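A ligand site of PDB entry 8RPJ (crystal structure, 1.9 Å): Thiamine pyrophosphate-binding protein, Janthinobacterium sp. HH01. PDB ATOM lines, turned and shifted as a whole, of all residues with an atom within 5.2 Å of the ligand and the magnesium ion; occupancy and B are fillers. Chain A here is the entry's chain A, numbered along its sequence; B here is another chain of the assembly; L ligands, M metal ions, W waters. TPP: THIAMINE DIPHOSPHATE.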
ATOM      1  N   ASP A 406      15.083   1.947   4.045  1.00  0.00           N
ATOM      2  CA  ASP A 406      14.069   1.518   5.004  1.00  0.00           C
ATOM      3  C   ASP A 406      12.830   1.122   4.204  1.00  0.00           C
ATOM      4  O   ASP A 406      12.929   0.762   3.025  1.00  0.00           O
ATOM      5  CB  ASP A 406      13.782   2.625   6.022  1.00  0.00           C
ATOM      6  CG  ASP A 406      13.480   2.072   7.413  1.00  0.00           C
ATOM      7  OD1 ASP A 406      14.409   1.859   8.212  1.00  0.00           O
ATOM      8  OD2 ASP A 406      12.281   1.829   7.702  1.00  0.00           O
ATOM      9  N   MET A 407      11.662   1.163   4.832  1.00  0.00           N
ATOM     10  CA  MET A 407      10.416   0.800   4.170  1.00  0.00           C
ATOM     11  C   MET A 407       9.782   2.054   3.579  1.00  0.00           C
ATOM     12  O   MET A 407      10.496   3.002   3.227  1.00  0.00           O
ATOM     13  CB  MET A 407       9.507   0.079   5.158  1.00  0.00           C
ATOM     14  CG  MET A 407      10.156  -1.155   5.782  1.00  0.00           C
ATOM     15  SD  MET A 407      10.549  -2.426   4.540  1.00  0.00           S
ATOM     16  CE  MET A 407      12.339  -2.468   4.629  1.00  0.00           C
ATOM     17  N   GLY A 408       8.459   2.073   3.451  1.00  0.00           N
ATOM     18  CA  GLY A 408       7.739   3.268   3.087  1.00  0.00           C
ATOM     19  C   GLY A 408       8.171   3.884   1.761  1.00  0.00           C
ATOM     20  O   GLY A 408       8.521   3.195   0.799  1.00  0.00           O
ATOM     21  N   THR A 409       8.132   5.220   1.723  1.00  0.00           N
ATOM     22  CA  THR A 409       8.476   5.940   0.500  1.00  0.00           C
ATOM     23  C   THR A 409       9.839   5.516  -0.034  1.00  0.00           C
ATOM     24  O   THR A 409      10.002   5.318  -1.246  1.00  0.00           O
ATOM     25  CB  THR A 409       8.482   7.446   0.755  1.00  0.00           C
ATOM     26  OG1 THR A 409       7.170   7.878   1.135  1.00  0.00           O
ATOM     27  CG2 THR A 409       8.944   8.209  -0.477  1.00  0.00           C
ATOM     28  N   ALA A 410      10.822   5.398   0.854  1.00  0.00           N
ATOM     29  CA  ALA A 410      12.164   5.022   0.413  1.00  0.00           C
ATOM     30  C   ALA A 410      12.140   3.689  -0.309  1.00  0.00           C
ATOM     31  O   ALA A 410      12.737   3.541  -1.378  1.00  0.00           O
ATOM     32  CB  ALA A 410      13.109   4.968   1.622  1.00  0.00           C
ATOM     33  N   GLY A 433      10.305  -7.069   5.848  1.00  0.00           N
ATOM     34  CA  GLY A 433       9.805  -5.735   5.615  1.00  0.00           C
ATOM     35  C   GLY A 433       9.706  -4.881   6.857  1.00  0.00           C
ATOM     36  O   GLY A 433       8.764  -4.107   6.993  1.00  0.00           O
ATOM     37  N   GLU A 434      10.669  -5.005   7.769  1.00  0.00           N
ATOM     38  CA  GLU A 434      10.588  -4.296   9.035  1.00  0.00           C
ATOM     39  C   GLU A 434      11.018  -2.843   8.874  1.00  0.00           C
ATOM     40  O   GLU A 434      12.038  -2.544   8.246  1.00  0.00           O
ATOM     41  CB  GLU A 434      11.455  -4.982  10.105  1.00  0.00           C
ATOM     42  CG  GLU A 434      12.963  -4.824   9.931  1.00  0.00           C
ATOM     43  CD  GLU A 434      13.586  -5.943   9.124  1.00  0.00           C
ATOM     44  OE1 GLU A 434      12.986  -6.370   8.116  1.00  0.00           O
ATOM     45  OE2 GLU A 434      14.696  -6.390   9.489  1.00  0.00           O
ATOM     46  N   MET A 435      10.235  -1.935   9.456  1.00  0.00           N
ATOM     47  CA  MET A 435      10.687  -0.573   9.664  1.00  0.00           C
ATOM     48  C   MET A 435      11.929  -0.579  10.546  1.00  0.00           C
ATOM     49  O   MET A 435      12.073  -1.408  11.450  1.00  0.00           O
ATOM     50  CB  MET A 435       9.602   0.261  10.311  1.00  0.00           C
ATOM     51  CG  MET A 435       8.388   0.455   9.456  1.00  0.00           C
ATOM     52  SD  MET A 435       7.065   1.197  10.419  1.00  0.00           S
ATOM     53  CE  MET A 435       7.722   2.835  10.688  1.00  0.00           C
ATOM     54  N   CYS A 459      12.936   7.217   6.293  1.00  0.00           N
ATOM     55  CA  CYS A 459      11.592   7.736   6.430  1.00  0.00           C
ATOM     56  C   CYS A 459      11.392   8.271   7.826  1.00  0.00           C
ATOM     57  O   CYS A 459      12.050   7.850   8.777  1.00  0.00           O
ATOM     58  CB  CYS A 459      10.549   6.649   6.161  1.00  0.00           C
ATOM     59  SG  CYS A 459      10.732   5.929   4.545  1.00  0.00           S
ATOM     60  N   ASP A 460      10.445   9.191   7.965  1.00  0.00           N
ATOM     61  CA  ASP A 460      10.228   9.809   9.267  1.00  0.00           C
ATOM     62  C   ASP A 460       9.753   8.776  10.280  1.00  0.00           C
ATOM     63  O   ASP A 460      10.174   8.800  11.434  1.00  0.00           O
ATOM     64  CB  ASP A 460       9.293  11.015   9.144  1.00  0.00           C
ATOM     65  CG  ASP A 460       7.969  10.725   8.439  1.00  0.00           C
ATOM     66  OD1 ASP A 460       7.728   9.612   7.925  1.00  0.00           O
ATOM     67  OD2 ASP A 460       7.142  11.669   8.421  1.00  0.00           O
ATOM     68  N   GLY A 461       8.932   7.817   9.864  1.00  0.00           N
ATOM     69  CA  GLY A 461       8.524   6.753  10.751  1.00  0.00           C
ATOM     70  C   GLY A 461       9.592   5.709  11.021  1.00  0.00           C
ATOM     71  O   GLY A 461       9.895   5.398  12.175  1.00  0.00           O
ATOM     72  N   GLY A 462      10.174   5.190   9.938  1.00  0.00           N
ATOM     73  CA  GLY A 462      11.193   4.161  10.072  1.00  0.00           C
ATOM     74  C   GLY A 462      12.433   4.636  10.817  1.00  0.00           C
ATOM     75  O   GLY A 462      13.099   3.838  11.484  1.00  0.00           O
ATOM     76  N   MET A 465      12.562   3.651  14.742  1.00  0.00           N
ATOM     77  CA  MET A 465      12.709   2.317  15.338  1.00  0.00           C
ATOM     78  C   MET A 465      14.145   2.061  15.799  1.00  0.00           C
ATOM     79  O   MET A 465      14.361   1.411  16.820  1.00  0.00           O
ATOM     80  CB  MET A 465      12.279   1.224  14.362  1.00  0.00           C
ATOM     81  CG  MET A 465      10.821   0.830  14.504  1.00  0.00           C
ATOM     82  SD  MET A 465       9.820   2.110  13.738  1.00  0.00           S
ATOM     83  CE  MET A 465       8.183   1.507  14.076  1.00  0.00           C
ATOM     84  N   PHE A 485      12.572  10.956   4.244  1.00  0.00           N
ATOM     85  CA  PHE A 485      11.338  11.439   3.622  1.00  0.00           C
ATOM     86  C   PHE A 485      10.322  11.802   4.699  1.00  0.00           C
ATOM     87  O   PHE A 485       9.798  10.922   5.394  1.00  0.00           O
ATOM     88  CB  PHE A 485      10.770  10.384   2.670  1.00  0.00           C
ATOM     89  CG  PHE A 485      11.576  10.240   1.417  1.00  0.00           C
ATOM     90  CD1 PHE A 485      11.435  11.140   0.379  1.00  0.00           C
ATOM     91  CD2 PHE A 485      12.507   9.220   1.301  1.00  0.00           C
ATOM     92  CE1 PHE A 485      12.180  11.022  -0.769  1.00  0.00           C
ATOM     93  CE2 PHE A 485      13.265   9.104   0.147  1.00  0.00           C
ATOM     94  CZ  PHE A 485      13.098  10.002  -0.879  1.00  0.00           C
ATOM     95  N   ASN A 487       6.707  13.027   5.665  1.00  0.00           N
ATOM     96  CA  ASN A 487       5.352  13.077   5.126  1.00  0.00           C
ATOM     97  C   ASN A 487       4.291  12.986   6.233  1.00  0.00           C
ATOM     98  O   ASN A 487       3.219  12.415   6.000  1.00  0.00           O
ATOM     99  CB  ASN A 487       5.128  11.978   4.072  1.00  0.00           C
ATOM    100  CG  ASN A 487       5.609  10.607   4.542  1.00  0.00           C
ATOM    101  OD1 ASN A 487       5.643  10.309   5.741  1.00  0.00           O
ATOM    102  ND2 ASN A 487       5.955   9.747   3.588  1.00  0.00           N
ATOM    103  N   GLY A 489       4.075  11.297   9.118  1.00  0.00           N
ATOM    104  CA  GLY A 489       3.741  10.009   9.678  1.00  0.00           C
ATOM    105  C   GLY A 489       3.826   8.850   8.724  1.00  0.00           C
ATOM    106  O   GLY A 489       4.775   8.740   7.941  1.00  0.00           O
ATOM    107  N   TYR A 490       2.810   7.972   8.762  1.00  0.00           N
ATOM    108  CA  TYR A 490       2.862   6.670   8.121  1.00  0.00           C
ATOM    109  C   TYR A 490       2.082   6.677   6.807  1.00  0.00           C
ATOM    110  O   TYR A 490       0.948   6.221   6.735  1.00  0.00           O
ATOM    111  CB  TYR A 490       2.271   5.621   9.054  1.00  0.00           C
ATOM    112  CG  TYR A 490       3.003   5.385  10.344  1.00  0.00           C
ATOM    113  CD1 TYR A 490       4.313   5.814  10.519  1.00  0.00           C
ATOM    114  CD2 TYR A 490       2.388   4.707  11.376  1.00  0.00           C
ATOM    115  CE1 TYR A 490       4.982   5.582  11.711  1.00  0.00           C
ATOM    116  CE2 TYR A 490       3.047   4.467  12.562  1.00  0.00           C
ATOM    117  CZ  TYR A 490       4.337   4.900  12.731  1.00  0.00           C
ATOM    118  OH  TYR A 490       4.983   4.651  13.919  1.00  0.00           O
ATOM    119  N   LEU A 491       2.723   7.162   5.745  1.00  0.00           N
ATOM    120  CA  LEU A 491       2.000   7.362   4.503  1.00  0.00           C
ATOM    121  C   LEU A 491       1.466   6.049   3.948  1.00  0.00           C
ATOM    122  O   LEU A 491       0.323   5.985   3.480  1.00  0.00           O
ATOM    123  CB  LEU A 491       2.891   8.060   3.492  1.00  0.00           C
ATOM    124  CG  LEU A 491       2.257   8.369   2.136  1.00  0.00           C
ATOM    125  CD1 LEU A 491       0.943   9.068   2.255  1.00  0.00           C
ATOM    126  CD2 LEU A 491       3.255   9.220   1.348  1.00  0.00           C
ATOM    127  N   MET A 492       2.266   4.987   3.980  1.00  0.00           N
ATOM    128  CA  MET A 492       1.786   3.732   3.427  1.00  0.00           C
ATOM    129  C   MET A 492       0.493   3.285   4.112  1.00  0.00           C
ATOM    130  O   MET A 492      -0.433   2.807   3.452  1.00  0.00           O
ATOM    131  CB  MET A 492       2.844   2.652   3.541  1.00  0.00           C
ATOM    132  CG  MET A 492       2.603   1.541   2.565  1.00  0.00           C
ATOM    133  SD  MET A 492       3.941   0.357   2.482  1.00  0.00           S
ATOM    134  CE  MET A 492       3.145  -0.945   1.556  1.00  0.00           C
ATOM    135  N   ILE A 493       0.417   3.453   5.436  1.00  0.00           N
ATOM    136  CA  ILE A 493      -0.783   3.005   6.132  1.00  0.00           C
ATOM    137  C   ILE A 493      -1.935   4.005   5.929  1.00  0.00           C
ATOM    138  O   ILE A 493      -3.099   3.598   5.914  1.00  0.00           O
ATOM    139  CB  ILE A 493      -0.489   2.772   7.623  1.00  0.00           C
ATOM    140  CG1 ILE A 493       0.731   1.849   7.794  1.00  0.00           C
ATOM    141  CG2 ILE A 493      -1.706   2.179   8.319  1.00  0.00           C
ATOM    142  CD1 ILE A 493       0.604   0.476   7.134  1.00  0.00           C
ATOM    143  N   PHE A 565       1.321   6.509  -3.795  1.00  0.00           N
ATOM    144  CA  PHE A 565       2.307   5.568  -4.299  1.00  0.00           C
ATOM    145  C   PHE A 565       1.680   4.888  -5.504  1.00  0.00           C
ATOM    146  O   PHE A 565       0.580   4.329  -5.415  1.00  0.00           O
ATOM    147  CB  PHE A 565       2.670   4.534  -3.235  1.00  0.00           C
ATOM    148  CG  PHE A 565       3.367   5.107  -2.042  1.00  0.00           C
ATOM    149  CD1 PHE A 565       4.402   6.023  -2.183  1.00  0.00           C
ATOM    150  CD2 PHE A 565       2.994   4.710  -0.768  1.00  0.00           C
ATOM    151  CE1 PHE A 565       5.045   6.528  -1.062  1.00  0.00           C
ATOM    152  CE2 PHE A 565       3.631   5.219   0.341  1.00  0.00           C
ATOM    153  CZ  PHE A 565       4.656   6.128   0.194  1.00  0.00           C
ATOM    154  N   ILE B  28       1.605  -0.229  17.597  1.00  0.00           N
ATOM    155  CA  ILE B  28       1.916   0.386  16.313  1.00  0.00           C
ATOM    156  C   ILE B  28       1.039  -0.274  15.261  1.00  0.00           C
ATOM    157  O   ILE B  28       0.883  -1.501  15.244  1.00  0.00           O
ATOM    158  CB  ILE B  28       3.407   0.263  15.961  1.00  0.00           C
ATOM    159  CG1 ILE B  28       4.263   0.873  17.080  1.00  0.00           C
ATOM    160  CG2 ILE B  28       3.718   0.939  14.616  1.00  0.00           C
ATOM    161  CD1 ILE B  28       5.760   0.941  16.790  1.00  0.00           C
ATOM    162  N   ILE B  29       0.490   0.546  14.379  1.00  0.00           N
ATOM    163  CA  ILE B  29      -0.422   0.080  13.354  1.00  0.00           C
ATOM    164  C   ILE B  29       0.341  -0.614  12.237  1.00  0.00           C
ATOM    165  O   ILE B  29       1.555  -0.446  12.055  1.00  0.00           O
ATOM    166  CB  ILE B  29      -1.247   1.264  12.816  1.00  0.00           C
ATOM    167  CG1 ILE B  29      -2.503   0.795  12.090  1.00  0.00           C
ATOM    168  CG2 ILE B  29      -0.379   2.123  11.904  1.00  0.00           C
ATOM    169  CD1 ILE B  29      -3.500   1.919  11.878  1.00  0.00           C
ATOM    170  N   GLY B  30      -0.386  -1.430  11.487  1.00  0.00           N
ATOM    171  CA  GLY B  30       0.081  -2.064  10.264  1.00  0.00           C
ATOM    172  C   GLY B  30      -1.115  -2.734   9.628  1.00  0.00           C
ATOM    173  O   GLY B  30      -2.203  -2.784  10.219  1.00  0.00           O
ATOM    174  N   GLU B  54       7.652  -1.323  19.129  1.00  0.00           N
ATOM    175  CA  GLU B  54       6.687  -2.196  19.802  1.00  0.00           C
ATOM    176  C   GLU B  54       7.182  -2.687  21.146  1.00  0.00           C
ATOM    177  O   GLU B  54       6.372  -3.010  22.033  1.00  0.00           O
ATOM    178  CB  GLU B  54       6.354  -3.375  18.873  1.00  0.00           C
ATOM    179  CG  GLU B  54       5.495  -3.003  17.659  1.00  0.00           C
ATOM    180  CD  GLU B  54       6.279  -2.555  16.432  1.00  0.00           C
ATOM    181  OE1 GLU B  54       7.509  -2.354  16.517  1.00  0.00           O
ATOM    182  OE2 GLU B  54       5.637  -2.398  15.374  1.00  0.00           O
ATOM    183  N   THR B  77       1.346  -5.668  15.117  1.00  0.00           N
ATOM    184  CA  THR B  77       1.025  -6.105  13.771  1.00  0.00           C
ATOM    185  C   THR B  77       1.892  -7.292  13.356  1.00  0.00           C
ATOM    186  O   THR B  77       2.732  -7.800  14.121  1.00  0.00           O
ATOM    187  CB  THR B  77       1.135  -4.939  12.776  1.00  0.00           C
ATOM    188  OG1 THR B  77       0.478  -5.307  11.553  1.00  0.00           O
ATOM    189  CG2 THR B  77       2.579  -4.568  12.469  1.00  0.00           C
ATOM    190  N   ALA B  80       7.512  -8.021  11.942  1.00  0.00           N
ATOM    191  CA  ALA B  80       8.365  -7.319  12.896  1.00  0.00           C
ATOM    192  C   ALA B  80       7.569  -6.571  13.949  1.00  0.00           C
ATOM    193  O   ALA B  80       8.116  -6.271  15.013  1.00  0.00           O
ATOM    194  CB  ALA B  80       9.288  -6.355  12.143  1.00  0.00           C
ATOM    195  N   GLY B  81       6.304  -6.256  13.689  1.00  0.00           N
ATOM    196  CA  GLY B  81       5.461  -5.737  14.751  1.00  0.00           C
ATOM    197  C   GLY B  81       5.367  -6.668  15.934  1.00  0.00           C
ATOM    198  O   GLY B  81       5.283  -6.218  17.088  1.00  0.00           O
ATOM    199  N   ASN B  84       9.208  -7.480  17.482  1.00  0.00           N
ATOM    200  CA  ASN B  84       9.702  -6.343  18.252  1.00  0.00           C
ATOM    201  C   ASN B  84       9.146  -6.301  19.660  1.00  0.00           C
ATOM    202  O   ASN B  84       9.717  -5.616  20.516  1.00  0.00           O
ATOM    203  CB  ASN B  84       9.352  -5.038  17.539  1.00  0.00           C
ATOM    204  CG  ASN B  84      10.402  -4.600  16.541  1.00  0.00           C
ATOM    205  OD1 ASN B  84      11.417  -5.277  16.337  1.00  0.00           O
ATOM    206  ND2 ASN B  84      10.159  -3.470  15.888  1.00  0.00           N
ATOM    207  N   GLN B 123       4.653 -11.730   5.035  1.00  0.00           N
ATOM    208  CA  GLN B 123       5.708 -11.494   6.009  1.00  0.00           C
ATOM    209  C   GLN B 123       5.363 -11.965   7.417  1.00  0.00           C
ATOM    210  O   GLN B 123       5.859 -11.404   8.399  1.00  0.00           O
ATOM    211  CB  GLN B 123       6.066  -9.994   6.064  1.00  0.00           C
ATOM    212  CG  GLN B 123       4.879  -9.067   6.258  1.00  0.00           C
ATOM    213  CD  GLN B 123       5.232  -7.620   6.000  1.00  0.00           C
ATOM    214  OE1 GLN B 123       5.928  -7.295   5.037  1.00  0.00           O
ATOM    215  NE2 GLN B 123       4.778  -6.727   6.877  1.00  0.00           N
HETATM  216  N1' TPP L   1       6.177  -2.118  12.824  1.00  0.00           N
HETATM  217  C2' TPP L   1       7.301  -2.588  12.242  1.00  0.00           C
HETATM  218  CM2 TPP L   1       8.466  -2.862  13.135  1.00  0.00           C
HETATM  219  N3' TPP L   1       7.454  -2.822  10.940  1.00  0.00           N
HETATM  220  C4' TPP L   1       6.411  -2.570  10.120  1.00  0.00           C
HETATM  221  N4' TPP L   1       6.590  -2.829   8.822  1.00  0.00           N
HETATM  222  C5' TPP L   1       5.186  -2.062  10.640  1.00  0.00           C
HETATM  223  C6' TPP L   1       5.157  -1.868  12.000  1.00  0.00           C
HETATM  224  C7' TPP L   1       3.973  -1.762   9.780  1.00  0.00           C
HETATM  225  N3  TPP L   1       4.209  -0.678   8.778  1.00  0.00           N
HETATM  226  C2  TPP L   1       4.461  -0.909   7.503  1.00  0.00           C
HETATM  227  S1  TPP L   1       4.675   0.513   6.637  1.00  0.00           S
HETATM  228  C5  TPP L   1       4.382   1.464   8.041  1.00  0.00           C
HETATM  229  C4  TPP L   1       4.149   0.675   9.110  1.00  0.00           C
HETATM  230  CM4 TPP L   1       3.867   1.114  10.505  1.00  0.00           C
HETATM  231  C6  TPP L   1       4.457   2.964   7.978  1.00  0.00           C
HETATM  232  C7  TPP L   1       5.780   3.436   7.444  1.00  0.00           C
HETATM  233  O7  TPP L   1       5.930   4.855   7.696  1.00  0.00           O
HETATM  234  PA  TPP L   1       7.210   5.667   7.301  1.00  0.00           P
HETATM  235  O1A TPP L   1       7.103   7.058   7.801  1.00  0.00           O
HETATM  236  O2A TPP L   1       8.424   4.848   7.685  1.00  0.00           O
HETATM  237  O3A TPP L   1       7.046   5.643   5.748  1.00  0.00           O
HETATM  238  PB  TPP L   1       6.083   6.222   4.648  1.00  0.00           P
HETATM  239  O1B TPP L   1       5.089   5.203   4.205  1.00  0.00           O
HETATM  240  O2B TPP L   1       7.001   6.771   3.564  1.00  0.00           O
HETATM  241  O3B TPP L   1       5.444   7.397   5.376  1.00  0.00           O
HETATM  242 MG    MG M   1       6.394   8.619   6.735  1.00  0.00          MG
HETATM  243  O   HOH W   1       4.589  -4.043   7.181  1.00  0.00           O
HETATM  244  O   HOH W   2       9.966   3.183   6.617  1.00  0.00           O
HETATM  245  O   HOH W   3       8.118   8.574   5.413  1.00  0.00           O
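CA of Gly 408 touches O1B of the ligand, at 3.5 Å. Glu 434 touches the ligand. Cys 459 touches the ligand. Tyr 490 touches the ligand (CD1 to O7, 3.4 Å). Ile 493 touches the ligand. Ile 29 of chain B touches the ligand (O to CM4, 3.2 Å). CA of Gly 30 of chain B touches C7' of the ligand, at 3.9 Å. CG2 of Thr 77 of chain B touches C6' of the ligand, 3.8 Å away. Ala 80 of chain B touches the ligand (CB to CM2, 3.7 Å). Asn 84 of chain B touches the ligand. Hydrophobic or aromatic side chains that line the ligand: Met 435, Tyr 490, Leu 491, Met 492, Ile 493 and Ala 80 of chain B. 21 residues have an atom within 4 Å of the ligand: Gly 408, Thr 409, Gly 433, Glu 434, Met 435, Cys 459, Asp 460, Gly 461, Gly 462, Asn 487, Gly 489, Tyr 490, Leu 491, Met 492, Ile 493, Ile 29 of chain B, Gly 30 of chain B, Glu 54 of chain B, Thr 77 of chain B, Ala 80 of chain B and Asn 84 of chain B. The nearest printed residue that does not touch the ligand is Gly 81 of chain B (4.1 Å).
Three residues have an atom within 4 Å of the magnesium ion: Asp 460, Asn 487 and Gly 489.
Water W3 lies within hydrogen-bond range of O2B of the ligand, O of Phe 485 and ND2 of Asn 487. Water W2 lies within hydrogen-bond range of O2A of the ligand (2.5 Å), OD2 of Asp 406 (2.9 Å), N of Met 407 (3.2 Å) and SG of Cys 459 (3.5 Å). Water W1 lies within hydrogen-bond range of NE2 of Gln 123 of chain B (2.7 Å) and N4' of the ligand (2.9 Å).
The backbone NH of Asp 460 lies within hydrogen-bond range of the backbone carbonyl oxygen of Phe 485 (3.2 Å). The side-chain amide nitrogen (ND2) of Asn 487 sits at hydrogen-bond distance from the side-chain hydroxyl (OG1) of Thr 409 (3.3 Å). The side-chain carboxylate (OE1) of Glu 54 of chain B is in hydrogen-bond range of the side-chain amide nitrogen (ND2) of Asn 84 of chain B, at 2.9 Å. The side-chain sulfur (SG) of Cys 459 sits at hydrogen-bond distance from the backbone NH (N) of Ala 410 (3.7 Å). The side-chain sulfur (SG) of Cys 459 is in hydrogen-bond range of the backbone carbonyl oxygen (O) of Met 407 (3.2 Å).
A nitrogen (N1') of the ligand sits at hydrogen-bond distance from the side-chain carboxylate (OE2) of Glu 54 of chain B (2.6 Å). The backbone NH (N) of Thr 409 lies within hydrogen-bond range of an oxygen (O2B) of the ligand (2.7 Å). OG1 of Thr 409 is in hydrogen-bond range of O2B of the ligand. The backbone NH of Leu 491 lies within hydrogen-bond range of an oxygen (O1B) of the ligand (3.4 Å). An oxygen (O1B) of the ligand sits at hydrogen-bond distance from the backbone NH (N) of Met 492 (2.8 Å). O1A of the ligand lies close to N of Gly 461 (2.9 Å). The backbone NH (N) of Gly 462 sits at hydrogen-bond distance from an oxygen (O2A) of the ligand (2.9 Å). O of Gly 433 lies within hydrogen-bond range of N4' of the ligand (3.1 Å). The backbone NH (N) of Met 435 is in hydrogen-bond range of a nitrogen (N3') of the ligand (3.3 Å).
The magnesium ion is bound by O1A of the ligand (2.0 Å). The magnesium ion is bound by the backbone carbonyl oxygen (O) of Gly 489 (2.0 Å). The magnesium ion is bound by OD1 of Asp 460, 2.0 Å away. O3B of the ligand is bound to the magnesium ion, at 2.1 Å. The side-chain amide oxygen (OD1) of Asn 487 is bound to the magnesium ion. The magnesium ion is bound by water W3, 2.2 Å away. The magnesium ion has six donor atoms within binding distance.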
